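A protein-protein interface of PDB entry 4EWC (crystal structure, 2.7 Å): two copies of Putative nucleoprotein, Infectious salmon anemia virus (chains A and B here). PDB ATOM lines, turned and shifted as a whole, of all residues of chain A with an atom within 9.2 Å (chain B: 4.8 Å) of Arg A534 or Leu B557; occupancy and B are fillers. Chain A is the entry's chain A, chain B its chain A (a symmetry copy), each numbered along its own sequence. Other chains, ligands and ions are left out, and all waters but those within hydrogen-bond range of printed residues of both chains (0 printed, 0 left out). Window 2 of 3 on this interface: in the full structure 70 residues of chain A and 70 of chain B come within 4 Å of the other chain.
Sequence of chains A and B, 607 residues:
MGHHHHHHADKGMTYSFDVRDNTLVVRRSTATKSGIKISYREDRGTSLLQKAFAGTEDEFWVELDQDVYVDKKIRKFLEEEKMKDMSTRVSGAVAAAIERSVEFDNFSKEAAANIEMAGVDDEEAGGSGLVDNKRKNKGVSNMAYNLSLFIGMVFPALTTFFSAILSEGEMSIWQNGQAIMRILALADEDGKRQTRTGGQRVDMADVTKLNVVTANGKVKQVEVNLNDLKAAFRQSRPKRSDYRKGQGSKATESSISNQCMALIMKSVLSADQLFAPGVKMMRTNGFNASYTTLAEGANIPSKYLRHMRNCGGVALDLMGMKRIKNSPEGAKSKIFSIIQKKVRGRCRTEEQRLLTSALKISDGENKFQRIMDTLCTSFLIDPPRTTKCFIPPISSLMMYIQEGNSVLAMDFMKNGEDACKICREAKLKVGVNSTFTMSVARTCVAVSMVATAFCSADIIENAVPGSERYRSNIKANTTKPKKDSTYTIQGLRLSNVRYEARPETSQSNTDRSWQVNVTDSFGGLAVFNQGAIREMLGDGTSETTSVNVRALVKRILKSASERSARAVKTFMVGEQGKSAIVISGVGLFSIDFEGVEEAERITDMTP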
ATOM      1  N   VAL A 516      -7.023  -1.379 -25.004  1.00  0.00           N
ATOM      2  CA  VAL A 516      -7.378  -2.649 -24.417  1.00  0.00           C
ATOM      3  C   VAL A 516      -6.706  -3.843 -25.102  1.00  0.00           C
ATOM      4  O   VAL A 516      -6.957  -4.991 -24.731  1.00  0.00           O
ATOM      5  CB  VAL A 516      -8.909  -2.832 -24.402  1.00  0.00           C
ATOM      6  CG1 VAL A 516      -9.540  -1.787 -23.499  1.00  0.00           C
ATOM      7  CG2 VAL A 516      -9.464  -2.720 -25.810  1.00  0.00           C
ATOM      8  N   PHE A 528      -4.919  -9.118 -25.496  1.00  0.00           N
ATOM      9  CA  PHE A 528      -6.012  -8.219 -25.164  1.00  0.00           C
ATOM     10  C   PHE A 528      -6.552  -8.450 -23.747  1.00  0.00           C
ATOM     11  O   PHE A 528      -6.338  -9.513 -23.165  1.00  0.00           O
ATOM     12  CB  PHE A 528      -7.114  -8.403 -26.210  1.00  0.00           C
ATOM     13  CG  PHE A 528      -7.576  -9.811 -26.339  1.00  0.00           C
ATOM     14  CD1 PHE A 528      -8.599 -10.296 -25.533  1.00  0.00           C
ATOM     15  CD2 PHE A 528      -6.982 -10.664 -27.258  1.00  0.00           C
ATOM     16  CE1 PHE A 528      -9.018 -11.611 -25.649  1.00  0.00           C
ATOM     17  CE2 PHE A 528      -7.401 -11.972 -27.376  1.00  0.00           C
ATOM     18  CZ  PHE A 528      -8.414 -12.443 -26.570  1.00  0.00           C
ATOM     19  N   ASN A 529      -7.228  -7.442 -23.196  1.00  0.00           N
ATOM     20  CA  ASN A 529      -7.832  -7.531 -21.863  1.00  0.00           C
ATOM     21  C   ASN A 529      -9.196  -8.239 -21.936  1.00  0.00           C
ATOM     22  O   ASN A 529     -10.193  -7.650 -22.379  1.00  0.00           O
ATOM     23  CB  ASN A 529      -8.002  -6.138 -21.292  1.00  0.00           C
ATOM     24  CG  ASN A 529      -8.597  -6.134 -19.896  1.00  0.00           C
ATOM     25  OD1 ASN A 529      -9.654  -6.718 -19.647  1.00  0.00           O
ATOM     26  ND2 ASN A 529      -7.924  -5.440 -18.972  1.00  0.00           N
ATOM     27  N   GLN A 530      -9.234  -9.498 -21.504  1.00  0.00           N
ATOM     28  CA  GLN A 530     -10.450 -10.297 -21.538  1.00  0.00           C
ATOM     29  C   GLN A 530     -11.688  -9.573 -20.982  1.00  0.00           C
ATOM     30  O   GLN A 530     -12.676  -9.408 -21.694  1.00  0.00           O
ATOM     31  CB  GLN A 530     -10.212 -11.641 -20.825  1.00  0.00           C
ATOM     32  CG  GLN A 530     -11.425 -12.570 -20.736  1.00  0.00           C
ATOM     33  CD  GLN A 530     -12.062 -12.876 -22.090  1.00  0.00           C
ATOM     34  OE1 GLN A 530     -11.478 -12.626 -23.144  1.00  0.00           O
ATOM     35  NE2 GLN A 530     -13.276 -13.423 -22.061  1.00  0.00           N
ATOM     36  N   GLY A 531     -11.610  -9.131 -19.726  1.00  0.00           N
ATOM     37  CA  GLY A 531     -12.683  -8.387 -19.094  1.00  0.00           C
ATOM     38  C   GLY A 531     -13.267  -7.266 -19.941  1.00  0.00           C
ATOM     39  O   GLY A 531     -14.475  -7.122 -20.022  1.00  0.00           O
ATOM     40  N   ALA A 532     -12.410  -6.477 -20.579  1.00  0.00           N
ATOM     41  CA  ALA A 532     -12.856  -5.374 -21.435  1.00  0.00           C
ATOM     42  C   ALA A 532     -13.552  -5.879 -22.708  1.00  0.00           C
ATOM     43  O   ALA A 532     -14.553  -5.319 -23.157  1.00  0.00           O
ATOM     44  CB  ALA A 532     -11.662  -4.461 -21.795  1.00  0.00           C
ATOM     45  N   ILE A 533     -13.005  -6.948 -23.270  1.00  0.00           N
ATOM     46  CA  ILE A 533     -13.518  -7.519 -24.495  1.00  0.00           C
ATOM     47  C   ILE A 533     -14.895  -8.136 -24.252  1.00  0.00           C
ATOM     48  O   ILE A 533     -15.751  -8.158 -25.141  1.00  0.00           O
ATOM     49  CB  ILE A 533     -12.534  -8.589 -25.053  1.00  0.00           C
ATOM     50  CG1 ILE A 533     -11.213  -7.933 -25.503  1.00  0.00           C
ATOM     51  CG2 ILE A 533     -13.174  -9.385 -26.175  1.00  0.00           C
ATOM     52  CD1 ILE A 533     -11.309  -7.106 -26.771  1.00  0.00           C
ATOM     53  N   ARG A 534     -15.102  -8.624 -23.034  1.00  0.00           N
ATOM     54  CA  ARG A 534     -16.346  -9.270 -22.672  1.00  0.00           C
ATOM     55  C   ARG A 534     -17.434  -8.218 -22.446  1.00  0.00           C
ATOM     56  O   ARG A 534     -18.606  -8.408 -22.834  1.00  0.00           O
ATOM     57  CB  ARG A 534     -16.151 -10.133 -21.421  1.00  0.00           C
ATOM     58  CG  ARG A 534     -17.454 -10.674 -20.828  1.00  0.00           C
ATOM     59  CD  ARG A 534     -17.206 -11.623 -19.667  1.00  0.00           C
ATOM     60  NE  ARG A 534     -16.416 -12.781 -20.084  1.00  0.00           N
ATOM     61  CZ  ARG A 534     -16.937 -13.918 -20.534  1.00  0.00           C
ATOM     62  NH1 ARG A 534     -18.254 -14.054 -20.630  1.00  0.00           N
ATOM     63  NH2 ARG A 534     -16.144 -14.919 -20.886  1.00  0.00           N
ATOM     64  N   GLU A 535     -17.042  -7.107 -21.829  1.00  0.00           N
ATOM     65  CA  GLU A 535     -17.936  -5.970 -21.660  1.00  0.00           C
ATOM     66  C   GLU A 535     -18.345  -5.387 -22.989  1.00  0.00           C
ATOM     67  O   GLU A 535     -19.518  -5.115 -23.218  1.00  0.00           O
ATOM     68  CB  GLU A 535     -17.272  -4.883 -20.817  1.00  0.00           C
ATOM     69  CG  GLU A 535     -17.073  -5.307 -19.381  1.00  0.00           C
ATOM     70  CD  GLU A 535     -16.600  -4.190 -18.497  1.00  0.00           C
ATOM     71  OE1 GLU A 535     -16.127  -3.158 -19.033  1.00  0.00           O
ATOM     72  OE2 GLU A 535     -16.707  -4.343 -17.260  1.00  0.00           O
ATOM     73  N   MET A 536     -17.376  -5.225 -23.878  1.00  0.00           N
ATOM     74  CA  MET A 536     -17.651  -4.732 -25.223  1.00  0.00           C
ATOM     75  C   MET A 536     -18.589  -5.629 -26.045  1.00  0.00           C
ATOM     76  O   MET A 536     -19.261  -5.145 -26.940  1.00  0.00           O
ATOM     77  CB  MET A 536     -16.331  -4.494 -25.970  1.00  0.00           C
ATOM     78  CG  MET A 536     -15.508  -3.421 -25.328  1.00  0.00           C
ATOM     79  SD  MET A 536     -13.851  -3.111 -26.277  1.00  0.00           S
ATOM     80  CE  MET A 536     -14.611  -2.247 -27.877  1.00  0.00           C
ATOM     81  N   LEU A 537     -18.647  -6.920 -25.732  1.00  0.00           N
ATOM     82  CA  LEU A 537     -19.515  -7.827 -26.484  1.00  0.00           C
ATOM     83  C   LEU A 537     -20.850  -8.179 -25.808  1.00  0.00           C
ATOM     84  O   LEU A 537     -21.302  -7.497 -24.884  1.00  0.00           O
ATOM     85  CB  LEU A 537     -18.770  -9.118 -26.857  1.00  0.00           C
ATOM     86  CG  LEU A 537     -17.542  -9.005 -27.767  1.00  0.00           C
ATOM     87  CD1 LEU A 537     -16.803 -10.319 -27.795  1.00  0.00           C
ATOM     88  CD2 LEU A 537     -17.946  -8.566 -29.171  1.00  0.00           C
ATOM     89  N   LEU A 557     -17.233 -15.599  -9.952  1.00  0.00           N
ATOM     90  CA  LEU A 557     -16.838 -15.562 -11.348  1.00  0.00           C
ATOM     91  C   LEU A 557     -17.217 -14.234 -12.010  1.00  0.00           C
ATOM     92  O   LEU A 557     -16.444 -13.664 -12.782  1.00  0.00           O
ATOM     93  CB  LEU A 557     -17.458 -16.736 -12.096  1.00  0.00           C
ATOM     94  CG  LEU A 557     -17.193 -16.778 -13.599  1.00  0.00           C
ATOM     95  CD1 LEU A 557     -15.704 -16.879 -13.885  1.00  0.00           C
ATOM     96  CD2 LEU A 557     -17.964 -17.933 -14.204  1.00  0.00           C
ATOM     97  N   LYS A 558     -18.409 -13.739 -11.699  1.00  0.00           N
ATOM     98  CA  LYS A 558     -18.866 -12.475 -12.258  1.00  0.00           C
ATOM     99  C   LYS A 558     -17.999 -11.341 -11.738  1.00  0.00           C
ATOM    100  O   LYS A 558     -17.538 -10.503 -12.517  1.00  0.00           O
ATOM    101  CB  LYS A 558     -20.352 -12.245 -11.931  1.00  0.00           C
ATOM    102  CG  LYS A 558     -20.935 -10.944 -12.492  1.00  0.00           C
ATOM    103  CD  LYS A 558     -20.537 -10.706 -13.945  1.00  0.00           C
ATOM    104  CE  LYS A 558     -21.155  -9.422 -14.494  1.00  0.00           C
ATOM    105  NZ  LYS A 558     -22.633  -9.545 -14.688  1.00  0.00           N
ATOM    106  N   ALA A 560     -14.965 -11.378 -10.496  1.00  0.00           N
ATOM    107  CA  ALA A 560     -13.655 -11.511 -11.106  1.00  0.00           C
ATOM    108  C   ALA A 560     -13.611 -10.785 -12.438  1.00  0.00           C
ATOM    109  O   ALA A 560     -12.736  -9.941 -12.670  1.00  0.00           O
ATOM    110  CB  ALA A 560     -13.332 -12.974 -11.310  1.00  0.00           C
ATOM    111  N   SER A 561     -14.553 -11.120 -13.316  1.00  0.00           N
ATOM    112  CA  SER A 561     -14.542 -10.549 -14.652  1.00  0.00           C
ATOM    113  C   SER A 561     -14.794  -9.057 -14.585  1.00  0.00           C
ATOM    114  O   SER A 561     -14.177  -8.281 -15.323  1.00  0.00           O
ATOM    115  CB  SER A 561     -15.566 -11.221 -15.560  1.00  0.00           C
ATOM    116  OG  SER A 561     -15.314 -10.865 -16.914  1.00  0.00           O
ATOM    117  N   GLU A 562     -15.694  -8.661 -13.690  1.00  0.00           N
ATOM    118  CA  GLU A 562     -16.018  -7.251 -13.511  1.00  0.00           C
ATOM    119  C   GLU A 562     -14.765  -6.461 -13.125  1.00  0.00           C
ATOM    120  O   GLU A 562     -14.512  -5.361 -13.629  1.00  0.00           O
ATOM    121  CB  GLU A 562     -17.114  -7.082 -12.450  1.00  0.00           C
ATOM    122  N   SER A 564     -11.387  -7.570 -13.482  1.00  0.00           N
ATOM    123  CA  SER A 564     -10.235  -7.708 -14.385  1.00  0.00           C
ATOM    124  C   SER A 564     -10.332  -6.815 -15.636  1.00  0.00           C
ATOM    125  O   SER A 564      -9.371  -6.708 -16.407  1.00  0.00           O
ATOM    126  CB  SER A 564     -10.008  -9.177 -14.789  1.00  0.00           C
ATOM    127  OG  SER A 564     -11.095  -9.684 -15.546  1.00  0.00           O
ATOM    128  N   ALA A 565     -11.488  -6.176 -15.817  1.00  0.00           N
ATOM    129  CA  ALA A 565     -11.757  -5.374 -17.005  1.00  0.00           C
ATOM    130  C   ALA A 565     -10.979  -4.061 -17.020  1.00  0.00           C
ATOM    131  O   ALA A 565     -10.729  -3.485 -18.079  1.00  0.00           O
ATOM    132  CB  ALA A 565     -13.244  -5.097 -17.120  1.00  0.00           C
ATOM    133  N   ARG B 534     -11.334 -18.313 -14.630  1.00  0.00           N
ATOM    134  CA  ARG B 534     -12.647 -18.731 -15.072  1.00  0.00           C
ATOM    135  C   ARG B 534     -12.655 -20.239 -15.332  1.00  0.00           C
ATOM    136  O   ARG B 534     -13.636 -20.944 -15.011  1.00  0.00           O
ATOM    137  CB  ARG B 534     -13.055 -17.957 -16.329  1.00  0.00           C
ATOM    138  CG  ARG B 534     -14.324 -18.486 -17.003  1.00  0.00           C
ATOM    139  CD  ARG B 534     -14.760 -17.615 -18.170  1.00  0.00           C
ATOM    140  NE  ARG B 534     -15.047 -16.248 -17.737  1.00  0.00           N
ATOM    141  CZ  ARG B 534     -16.244 -15.825 -17.340  1.00  0.00           C
ATOM    142  NH1 ARG B 534     -17.272 -16.664 -17.318  1.00  0.00           N
ATOM    143  NH2 ARG B 534     -16.414 -14.565 -16.970  1.00  0.00           N
ATOM    144  N   VAL B 553     -21.761 -13.821 -31.711  1.00  0.00           N
ATOM    145  CA  VAL B 553     -21.303 -13.143 -30.504  1.00  0.00           C
ATOM    146  C   VAL B 553     -20.885 -14.123 -29.417  1.00  0.00           C
ATOM    147  O   VAL B 553     -19.781 -14.037 -28.870  1.00  0.00           O
ATOM    148  CB  VAL B 553     -22.386 -12.210 -29.925  1.00  0.00           C
ATOM    149  CG1 VAL B 553     -21.944 -11.661 -28.577  1.00  0.00           C
ATOM    150  CG2 VAL B 553     -22.695 -11.079 -30.902  1.00  0.00           C
ATOM    151  N   LYS B 554     -21.774 -15.062 -29.118  1.00  0.00           N
ATOM    152  CA  LYS B 554     -21.516 -16.096 -28.123  1.00  0.00           C
ATOM    153  C   LYS B 554     -20.212 -16.860 -28.389  1.00  0.00           C
ATOM    154  O   LYS B 554     -19.410 -17.066 -27.477  1.00  0.00           O
ATOM    155  CB  LYS B 554     -22.700 -17.071 -28.073  1.00  0.00           C
ATOM    156  N   ARG B 555     -20.010 -17.272 -29.641  1.00  0.00           N
ATOM    157  CA  ARG B 555     -18.808 -17.997 -30.030  1.00  0.00           C
ATOM    158  C   ARG B 555     -17.552 -17.164 -29.805  1.00  0.00           C
ATOM    159  O   ARG B 555     -16.609 -17.602 -29.139  1.00  0.00           O
ATOM    160  CB  ARG B 555     -18.888 -18.441 -31.497  1.00  0.00           C
ATOM    161  CG  ARG B 555     -19.788 -19.637 -31.714  1.00  0.00           C
ATOM    162  CD  ARG B 555     -19.895 -20.016 -33.176  1.00  0.00           C
ATOM    163  NE  ARG B 555     -21.234 -20.489 -33.476  1.00  0.00           N
ATOM    164  CZ  ARG B 555     -22.002 -20.022 -34.456  1.00  0.00           C
ATOM    165  NH1 ARG B 555     -21.558 -19.075 -35.275  1.00  0.00           N
ATOM    166  NH2 ARG B 555     -23.221 -20.516 -34.619  1.00  0.00           N
ATOM    167  N   ILE B 556     -17.557 -15.963 -30.373  1.00  0.00           N
ATOM    168  CA  ILE B 556     -16.449 -15.026 -30.251  1.00  0.00           C
ATOM    169  C   ILE B 556     -16.067 -14.824 -28.794  1.00  0.00           C
ATOM    170  O   ILE B 556     -14.885 -14.868 -28.436  1.00  0.00           O
ATOM    171  CB  ILE B 556     -16.816 -13.662 -30.834  1.00  0.00           C
ATOM    172  CG1 ILE B 556     -17.411 -13.817 -32.226  1.00  0.00           C
ATOM    173  CG2 ILE B 556     -15.594 -12.776 -30.889  1.00  0.00           C
ATOM    174  CD1 ILE B 556     -17.803 -12.510 -32.857  1.00  0.00           C
ATOM    175  N   LEU B 557     -17.080 -14.615 -27.958  1.00  0.00           N
ATOM    176  CA  LEU B 557     -16.850 -14.392 -26.542  1.00  0.00           C
ATOM    177  C   LEU B 557     -16.211 -15.612 -25.872  1.00  0.00           C
ATOM    178  O   LEU B 557     -15.304 -15.484 -25.047  1.00  0.00           O
ATOM    179  CB  LEU B 557     -18.158 -14.020 -25.854  1.00  0.00           C
ATOM    180  CG  LEU B 557     -18.082 -13.836 -24.341  1.00  0.00           C
ATOM    181  CD1 LEU B 557     -17.120 -12.716 -23.979  1.00  0.00           C
ATOM    182  CD2 LEU B 557     -19.475 -13.581 -23.804  1.00  0.00           C
ATOM    183  N   LYS B 558     -16.682 -16.798 -26.235  1.00  0.00           N
ATOM    184  CA  LYS B 558     -16.138 -18.026 -25.674  1.00  0.00           C
ATOM    185  C   LYS B 558     -14.696 -18.200 -26.121  1.00  0.00           C
ATOM    186  O   LYS B 558     -13.820 -18.482 -25.301  1.00  0.00           O
ATOM    187  CB  LYS B 558     -17.002 -19.235 -26.074  1.00  0.00           C
ATOM    188  CG  LYS B 558     -16.521 -20.578 -25.516  1.00  0.00           C
ATOM    189  CD  LYS B 558     -16.149 -20.495 -24.039  1.00  0.00           C
ATOM    190  CE  LYS B 558     -15.703 -21.851 -23.495  1.00  0.00           C
ATOM    191  NZ  LYS B 558     -16.841 -22.816 -23.383  1.00  0.00           N
ATOM    192  N   SER B 559     -14.465 -18.011 -27.421  1.00  0.00           N
ATOM    193  CA  SER B 559     -13.139 -18.166 -28.036  1.00  0.00           C
ATOM    194  C   SER B 559     -12.107 -17.247 -27.399  1.00  0.00           C
ATOM    195  O   SER B 559     -10.969 -17.656 -27.125  1.00  0.00           O
ATOM    196  CB  SER B 559     -13.208 -17.842 -29.526  1.00  0.00           C
ATOM    197  OG  SER B 559     -14.160 -18.649 -30.197  1.00  0.00           O
ATOM    198  N   ALA B 560     -12.522 -15.996 -27.201  1.00  0.00           N
ATOM    199  CA  ALA B 560     -11.727 -14.988 -26.525  1.00  0.00           C
ATOM    200  C   ALA B 560     -11.253 -15.498 -25.177  1.00  0.00           C
ATOM    201  O   ALA B 560     -10.051 -15.478 -24.880  1.00  0.00           O
ATOM    202  CB  ALA B 560     -12.548 -13.732 -26.336  1.00  0.00           C
ATOM    203  N   SER B 561     -12.199 -15.949 -24.358  1.00  0.00           N
ATOM    204  CA  SER B 561     -11.858 -16.373 -23.010  1.00  0.00           C
ATOM    205  C   SER B 561     -10.974 -17.603 -23.058  1.00  0.00           C
ATOM    206  O   SER B 561     -10.030 -17.729 -22.272  1.00  0.00           O
ATOM    207  CB  SER B 561     -13.103 -16.646 -22.174  1.00  0.00           C
ATOM    208  OG  SER B 561     -12.746 -16.748 -20.801  1.00  0.00           O
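Of chain B, only Arg B534, Leu B557 and Ser B561 come within 4 Å of Arg A534. Of the printed residues of chain A, Leu B557 touches Arg A534. Of the printed residues of chain A, Arg B534 touches Arg A534 (3.6 Å), Leu A557 (3.4 Å) and Ser A561 (3.7 Å). Of the printed residues of chain A, Ala B560 touches Phe A528 (3.8 Å) and Gln A530 (3.5 Å). Of the printed residues of chain A, Ser B561 touches Gln A530 (3.2 Å) and Arg A534 (3.7 Å). Of the printed residues of chain B, Ser A561 touches Arg B534 (3.7 Å). Of the printed residues of chain B, Phe A528 touches Ala B560. The nearest residue of chain A that does not touch Leu B557 is Gln A530 (4.2 Å). The nearest printed residue of chain B that does not touch Phe A528 is Ser B561 (5.5 Å).
Arg B534 touches its own counterpart, Arg A534. Arg A534 touches Leu B557, and with the chains exchanged Leu A557 touches Arg B534. Arg A534 touches Ser B561, and with the chains exchanged Ser A561 touches Arg B534. Positions printed for both chains: 534, 557, 558, 560 and 561.
Phe A528 touches Ala B560. OE1 of Gln A530 touches C of Ala B560, 3.5 Å away. Gln A530 touches Ser B561. NE of Arg A534 touches NH2 of Arg B534, 3.6 Å away. CD2 of Leu B557 touches NH1 of Arg A534, at 3.4 Å. Arg A534 touches Ser B561 (NH2 to CB, 3.7 Å). Leu A557 touches Arg B534 (CD2 to NH1, 3.4 Å). Ser A561 touches Arg B534.
Hydrophobic or aromatic side chains of chain A that line the printed part of chain B: Phe A528 and Leu A557. Hydrophobic or aromatic side chains of chain B within 4 Å of the printed part of chain A: Leu B557 and Ala B560. Among the printed residues, no Asp or Glu carboxylate lies within 4 Å of a Lys or Arg side-chain nitrogen of the other chain.
NH2 of Arg A534 sits close to NE2 of Gln A530 (3.4 Å). The side-chain hydroxyl of Ser A564 sits at hydrogen-bond distance from the backbone carbonyl oxygen of Ser A561 (3.4 Å).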
